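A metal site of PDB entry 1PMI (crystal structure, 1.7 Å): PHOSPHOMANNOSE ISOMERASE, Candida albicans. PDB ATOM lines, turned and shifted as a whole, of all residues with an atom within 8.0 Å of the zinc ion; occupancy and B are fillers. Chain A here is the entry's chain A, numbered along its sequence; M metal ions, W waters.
The zinc ion is bound by a ring nitrogen (NE2) of His 284 (2.1 Å), a ring nitrogen (NE2) of His 112 (2.1 Å), the side-chain amide oxygen (OE1) of Gln 110 (2.1 Å), the side-chain carboxylate (OE1) of Glu 137 (2.2 Å) and water W1 (2.2 Å).
The zinc ion has five donor atoms within binding distance.
Water W1 lies within hydrogen-bond range of the side-chain hydroxyl of Tyr 286 and the side-chain carboxylate of Glu 137.
Within 4 Å of the zinc ion: Gln 110, His 112, Glu 137 and His 284.
OE2 of Glu 137 is in salt-bridge range of NZ of Lys 135 (2.8 Å).
O of Glu 137 lies within hydrogen-bond range of N of Leu 278 (2.8 Å).
NE2 of Gln 110 lies within hydrogen-bond range of OG of Ser 108, at 3.0 Å.
ND1 of His 284 sits at hydrogen-bond distance from O of Asp 282, at 2.9 Å.
A ring nitrogen (ND1) of His 112 lies within hydrogen-bond range of the backbone carbonyl oxygen (O) of Asn 300 (2.8 Å).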
ATOM      1  N   SER A 108     -25.453  -1.038  -5.448  1.00  0.00           N
ATOM      2  CA  SER A 108     -24.854   0.005  -6.278  1.00  0.00           C
ATOM      3  C   SER A 108     -24.768  -0.378  -7.742  1.00  0.00           C
ATOM      4  O   SER A 108     -24.530  -1.558  -8.100  1.00  0.00           O
ATOM      5  CB  SER A 108     -23.440   0.418  -5.773  1.00  0.00           C
ATOM      6  OG  SER A 108     -22.595  -0.787  -5.948  1.00  0.00           O
ATOM      7  N   ILE A 109     -24.933   0.687  -8.564  1.00  0.00           N
ATOM      8  CA  ILE A 109     -24.636   0.574  -9.988  1.00  0.00           C
ATOM      9  C   ILE A 109     -23.122   0.459 -10.086  1.00  0.00           C
ATOM     10  O   ILE A 109     -22.398   1.252  -9.427  1.00  0.00           O
ATOM     11  CB  ILE A 109     -25.190   1.741 -10.841  1.00  0.00           C
ATOM     12  CG1 ILE A 109     -26.687   1.940 -10.607  1.00  0.00           C
ATOM     13  CG2 ILE A 109     -24.798   1.456 -12.350  1.00  0.00           C
ATOM     14  CD1 ILE A 109     -27.286   3.235 -11.164  1.00  0.00           C
ATOM     15  N   GLN A 110     -22.614  -0.594 -10.730  1.00  0.00           N
ATOM     16  CA  GLN A 110     -21.147  -0.852 -10.664  1.00  0.00           C
ATOM     17  C   GLN A 110     -20.641  -1.547 -11.885  1.00  0.00           C
ATOM     18  O   GLN A 110     -21.411  -2.051 -12.718  1.00  0.00           O
ATOM     19  CB  GLN A 110     -20.895  -1.694  -9.387  1.00  0.00           C
ATOM     20  CG  GLN A 110     -21.749  -3.029  -9.579  1.00  0.00           C
ATOM     21  CD  GLN A 110     -21.578  -3.930  -8.401  1.00  0.00           C
ATOM     22  OE1 GLN A 110     -21.187  -5.104  -8.511  1.00  0.00           O
ATOM     23  NE2 GLN A 110     -21.873  -3.468  -7.200  1.00  0.00           N
ATOM     24  N   ALA A 111     -19.325  -1.490 -12.021  1.00  0.00           N
ATOM     25  CA  ALA A 111     -18.599  -2.214 -13.096  1.00  0.00           C
ATOM     26  C   ALA A 111     -17.251  -2.654 -12.486  1.00  0.00           C
ATOM     27  O   ALA A 111     -16.774  -2.149 -11.470  1.00  0.00           O
ATOM     28  CB  ALA A 111     -18.425  -1.418 -14.337  1.00  0.00           C
ATOM     29  N   HIS A 112     -16.704  -3.727 -13.097  1.00  0.00           N
ATOM     30  CA  HIS A 112     -15.460  -4.343 -12.614  1.00  0.00           C
ATOM     31  C   HIS A 112     -14.436  -4.327 -13.750  1.00  0.00           C
ATOM     32  O   HIS A 112     -14.798  -4.471 -14.930  1.00  0.00           O
ATOM     33  CB  HIS A 112     -15.651  -5.780 -12.103  1.00  0.00           C
ATOM     34  CG  HIS A 112     -16.850  -5.870 -11.176  1.00  0.00           C
ATOM     35  ND1 HIS A 112     -16.851  -5.450  -9.892  1.00  0.00           N
ATOM     36  CD2 HIS A 112     -18.104  -6.315 -11.464  1.00  0.00           C
ATOM     37  CE1 HIS A 112     -18.079  -5.644  -9.369  1.00  0.00           C
ATOM     38  NE2 HIS A 112     -18.838  -6.129 -10.315  1.00  0.00           N
ATOM     39  N   LYS A 135     -13.013  -9.282 -11.726  1.00  0.00           N
ATOM     40  CA  LYS A 135     -14.076  -9.791 -10.840  1.00  0.00           C
ATOM     41  C   LYS A 135     -15.330 -10.205 -11.610  1.00  0.00           C
ATOM     42  O   LYS A 135     -16.384  -9.552 -11.482  1.00  0.00           O
ATOM     43  CB  LYS A 135     -14.483  -8.768  -9.779  1.00  0.00           C
ATOM     44  CG  LYS A 135     -15.332  -9.433  -8.699  1.00  0.00           C
ATOM     45  CD  LYS A 135     -16.056  -8.390  -7.844  1.00  0.00           C
ATOM     46  CE  LYS A 135     -16.909  -9.178  -6.816  1.00  0.00           C
ATOM     47  NZ  LYS A 135     -17.936  -8.296  -6.248  1.00  0.00           N
ATOM     48  N   PRO A 136     -15.220 -11.283 -12.368  1.00  0.00           N
ATOM     49  CA  PRO A 136     -16.335 -11.875 -13.080  1.00  0.00           C
ATOM     50  C   PRO A 136     -17.407 -12.264 -12.089  1.00  0.00           C
ATOM     51  O   PRO A 136     -17.014 -12.755 -10.961  1.00  0.00           O
ATOM     52  CB  PRO A 136     -15.713 -13.076 -13.802  1.00  0.00           C
ATOM     53  CG  PRO A 136     -14.566 -13.492 -12.849  1.00  0.00           C
ATOM     54  CD  PRO A 136     -13.959 -12.123 -12.481  1.00  0.00           C
ATOM     55  N   GLU A 137     -18.665 -12.083 -12.371  1.00  0.00           N
ATOM     56  CA  GLU A 137     -19.774 -12.476 -11.495  1.00  0.00           C
ATOM     57  C   GLU A 137     -20.864 -13.155 -12.316  1.00  0.00           C
ATOM     58  O   GLU A 137     -20.954 -12.845 -13.536  1.00  0.00           O
ATOM     59  CB  GLU A 137     -20.377 -11.281 -10.762  1.00  0.00           C
ATOM     60  CG  GLU A 137     -19.357 -10.567  -9.778  1.00  0.00           C
ATOM     61  CD  GLU A 137     -19.905  -9.111  -9.571  1.00  0.00           C
ATOM     62  OE1 GLU A 137     -20.473  -8.643 -10.540  1.00  0.00           O
ATOM     63  OE2 GLU A 137     -19.712  -8.665  -8.445  1.00  0.00           O
ATOM     64  N   MET A 138     -21.622 -14.070 -11.762  1.00  0.00           N
ATOM     65  CA  MET A 138     -22.755 -14.688 -12.520  1.00  0.00           C
ATOM     66  C   MET A 138     -23.918 -14.725 -11.564  1.00  0.00           C
ATOM     67  O   MET A 138     -23.647 -15.139 -10.386  1.00  0.00           O
ATOM     68  CB  MET A 138     -22.348 -16.075 -13.071  1.00  0.00           C
ATOM     69  CG  MET A 138     -23.482 -16.639 -13.940  1.00  0.00           C
ATOM     70  SD  MET A 138     -22.700 -18.269 -14.651  1.00  0.00           S
ATOM     71  CE  MET A 138     -22.590 -19.116 -13.097  1.00  0.00           C
ATOM     72  N   LEU A 278     -22.044 -11.262 -15.540  1.00  0.00           N
ATOM     73  CA  LEU A 278     -21.651  -9.821 -15.440  1.00  0.00           C
ATOM     74  C   LEU A 278     -20.194  -9.722 -15.905  1.00  0.00           C
ATOM     75  O   LEU A 278     -19.254  -9.903 -15.092  1.00  0.00           O
ATOM     76  CB  LEU A 278     -21.932  -9.334 -14.058  1.00  0.00           C
ATOM     77  CG  LEU A 278     -23.288  -9.245 -13.403  1.00  0.00           C
ATOM     78  CD1 LEU A 278     -24.318  -8.726 -14.445  1.00  0.00           C
ATOM     79  CD2 LEU A 278     -23.760 -10.578 -12.846  1.00  0.00           C
ATOM     80  N   GLN A 279     -20.013  -9.437 -17.180  1.00  0.00           N
ATOM     81  CA  GLN A 279     -18.638  -9.332 -17.738  1.00  0.00           C
ATOM     82  C   GLN A 279     -17.946  -8.081 -17.256  1.00  0.00           C
ATOM     83  O   GLN A 279     -18.615  -7.123 -16.765  1.00  0.00           O
ATOM     84  CB  GLN A 279     -18.716  -9.350 -19.273  1.00  0.00           C
ATOM     85  CG  GLN A 279     -19.536  -8.084 -19.643  1.00  0.00           C
ATOM     86  CD  GLN A 279     -20.147  -8.163 -20.993  1.00  0.00           C
ATOM     87  OE1 GLN A 279     -19.525  -8.639 -21.967  1.00  0.00           O
ATOM     88  NE2 GLN A 279     -21.399  -7.702 -21.100  1.00  0.00           N
ATOM     89  N   ASP A 282     -18.719  -3.434 -17.877  1.00  0.00           N
ATOM     90  CA  ASP A 282     -20.145  -3.438 -18.220  1.00  0.00           C
ATOM     91  C   ASP A 282     -20.963  -3.109 -16.974  1.00  0.00           C
ATOM     92  O   ASP A 282     -20.828  -3.775 -15.942  1.00  0.00           O
ATOM     93  CB  ASP A 282     -20.462  -4.818 -18.852  1.00  0.00           C
ATOM     94  CG  ASP A 282     -21.851  -4.768 -19.492  1.00  0.00           C
ATOM     95  OD1 ASP A 282     -22.019  -3.999 -20.430  1.00  0.00           O
ATOM     96  OD2 ASP A 282     -22.723  -5.433 -18.908  1.00  0.00           O
ATOM     97  N   PRO A 283     -21.763  -2.047 -17.037  1.00  0.00           N
ATOM     98  CA  PRO A 283     -22.523  -1.575 -15.885  1.00  0.00           C
ATOM     99  C   PRO A 283     -23.705  -2.438 -15.552  1.00  0.00           C
ATOM    100  O   PRO A 283     -24.441  -2.865 -16.464  1.00  0.00           O
ATOM    101  CB  PRO A 283     -22.906  -0.142 -16.260  1.00  0.00           C
ATOM    102  CG  PRO A 283     -23.022  -0.203 -17.797  1.00  0.00           C
ATOM    103  CD  PRO A 283     -21.991  -1.211 -18.249  1.00  0.00           C
ATOM    104  N   HIS A 284     -23.972  -2.610 -14.267  1.00  0.00           N
ATOM    105  CA  HIS A 284     -25.062  -3.476 -13.795  1.00  0.00           C
ATOM    106  C   HIS A 284     -25.397  -3.108 -12.373  1.00  0.00           C
ATOM    107  O   HIS A 284     -24.572  -2.411 -11.721  1.00  0.00           O
ATOM    108  CB  HIS A 284     -24.716  -5.003 -13.851  1.00  0.00           C
ATOM    109  CG  HIS A 284     -23.421  -5.335 -13.159  1.00  0.00           C
ATOM    110  ND1 HIS A 284     -22.189  -5.149 -13.770  1.00  0.00           N
ATOM    111  CD2 HIS A 284     -23.158  -5.775 -11.919  1.00  0.00           C
ATOM    112  CE1 HIS A 284     -21.215  -5.454 -12.906  1.00  0.00           C
ATOM    113  NE2 HIS A 284     -21.788  -5.883 -11.775  1.00  0.00           N
ATOM    114  N   ALA A 285     -26.541  -3.547 -11.901  1.00  0.00           N
ATOM    115  CA  ALA A 285     -26.940  -3.424 -10.483  1.00  0.00           C
ATOM    116  C   ALA A 285     -27.954  -4.509 -10.148  1.00  0.00           C
ATOM    117  O   ALA A 285     -28.769  -4.898 -11.029  1.00  0.00           O
ATOM    118  CB  ALA A 285     -27.507  -2.035 -10.145  1.00  0.00           C
ATOM    119  N   TYR A 286     -27.949  -4.958  -8.892  1.00  0.00           N
ATOM    120  CA  TYR A 286     -29.008  -5.860  -8.433  1.00  0.00           C
ATOM    121  C   TYR A 286     -30.107  -4.984  -7.779  1.00  0.00           C
ATOM    122  O   TYR A 286     -29.784  -4.215  -6.869  1.00  0.00           O
ATOM    123  CB  TYR A 286     -28.528  -6.963  -7.475  1.00  0.00           C
ATOM    124  CG  TYR A 286     -27.352  -7.778  -7.955  1.00  0.00           C
ATOM    125  CD1 TYR A 286     -26.986  -7.860  -9.308  1.00  0.00           C
ATOM    126  CD2 TYR A 286     -26.610  -8.498  -7.026  1.00  0.00           C
ATOM    127  CE1 TYR A 286     -25.882  -8.612  -9.720  1.00  0.00           C
ATOM    128  CE2 TYR A 286     -25.489  -9.280  -7.409  1.00  0.00           C
ATOM    129  CZ  TYR A 286     -25.150  -9.315  -8.768  1.00  0.00           C
ATOM    130  OH  TYR A 286     -24.036 -10.069  -9.110  1.00  0.00           O
ATOM    131  N   GLU A 293     -25.231 -16.536  -6.564  1.00  0.00           N
ATOM    132  CA  GLU A 293     -24.171 -15.715  -7.159  1.00  0.00           C
ATOM    133  C   GLU A 293     -22.811 -16.419  -7.086  1.00  0.00           C
ATOM    134  O   GLU A 293     -22.428 -16.974  -6.034  1.00  0.00           O
ATOM    135  CB  GLU A 293     -24.017 -14.353  -6.483  1.00  0.00           C
ATOM    136  CG  GLU A 293     -23.071 -13.373  -7.263  1.00  0.00           C
ATOM    137  CD  GLU A 293     -22.802 -12.103  -6.457  1.00  0.00           C
ATOM    138  OE1 GLU A 293     -22.643 -12.196  -5.238  1.00  0.00           O
ATOM    139  OE2 GLU A 293     -22.814 -11.056  -7.114  1.00  0.00           O
ATOM    140  N   MET A 295     -18.585 -15.881  -8.108  1.00  0.00           N
ATOM    141  CA  MET A 295     -17.608 -14.833  -8.531  1.00  0.00           C
ATOM    142  C   MET A 295     -16.204 -15.195  -8.211  1.00  0.00           C
ATOM    143  O   MET A 295     -15.978 -16.151  -7.402  1.00  0.00           O
ATOM    144  CB  MET A 295     -18.071 -13.515  -7.800  1.00  0.00           C
ATOM    145  CG  MET A 295     -17.705 -13.699  -6.335  1.00  0.00           C
ATOM    146  SD  MET A 295     -18.602 -12.446  -5.363  1.00  0.00           S
ATOM    147  CE  MET A 295     -17.329 -12.095  -4.119  1.00  0.00           C
ATOM    148  N   ASN A 300     -12.467  -5.401  -6.348  1.00  0.00           N
ATOM    149  CA  ASN A 300     -12.427  -4.279  -7.323  1.00  0.00           C
ATOM    150  C   ASN A 300     -13.814  -3.954  -7.855  1.00  0.00           C
ATOM    151  O   ASN A 300     -14.430  -4.814  -8.546  1.00  0.00           O
ATOM    152  CB  ASN A 300     -11.446  -4.617  -8.443  1.00  0.00           C
ATOM    153  CG  ASN A 300     -10.012  -4.432  -7.940  1.00  0.00           C
ATOM    154  OD1 ASN A 300      -9.875  -3.909  -6.819  1.00  0.00           O
ATOM    155  ND2 ASN A 300      -9.067  -4.859  -8.772  1.00  0.00           N
ATOM    156  N   VAL A 301     -14.270  -2.774  -7.488  1.00  0.00           N
ATOM    157  CA  VAL A 301     -15.574  -2.280  -7.924  1.00  0.00           C
ATOM    158  C   VAL A 301     -15.392  -0.787  -8.236  1.00  0.00           C
ATOM    159  O   VAL A 301     -14.774  -0.104  -7.432  1.00  0.00           O
ATOM    160  CB  VAL A 301     -16.695  -2.477  -6.911  1.00  0.00           C
ATOM    161  CG1 VAL A 301     -18.106  -2.310  -7.583  1.00  0.00           C
ATOM    162  CG2 VAL A 301     -16.638  -3.763  -6.168  1.00  0.00           C
ATOM    163  N   VAL A 302     -15.982  -0.428  -9.379  1.00  0.00           N
ATOM    164  CA  VAL A 302     -16.096   0.987  -9.759  1.00  0.00           C
ATOM    165  C   VAL A 302     -17.621   1.280  -9.655  1.00  0.00           C
ATOM    166  O   VAL A 302     -18.388   0.528 -10.295  1.00  0.00           O
ATOM    167  CB  VAL A 302     -15.482   1.290 -11.112  1.00  0.00           C
ATOM    168  CG1 VAL A 302     -15.549   2.821 -11.425  1.00  0.00           C
ATOM    169  CG2 VAL A 302     -14.058   0.829 -11.300  1.00  0.00           C
HETATM  170 ZN    ZN M   1     -20.907  -6.599 -10.028  1.00  0.00          ZN
HETATM  171  O   HOH W   1     -22.821  -7.319  -9.251  1.00  0.00           O
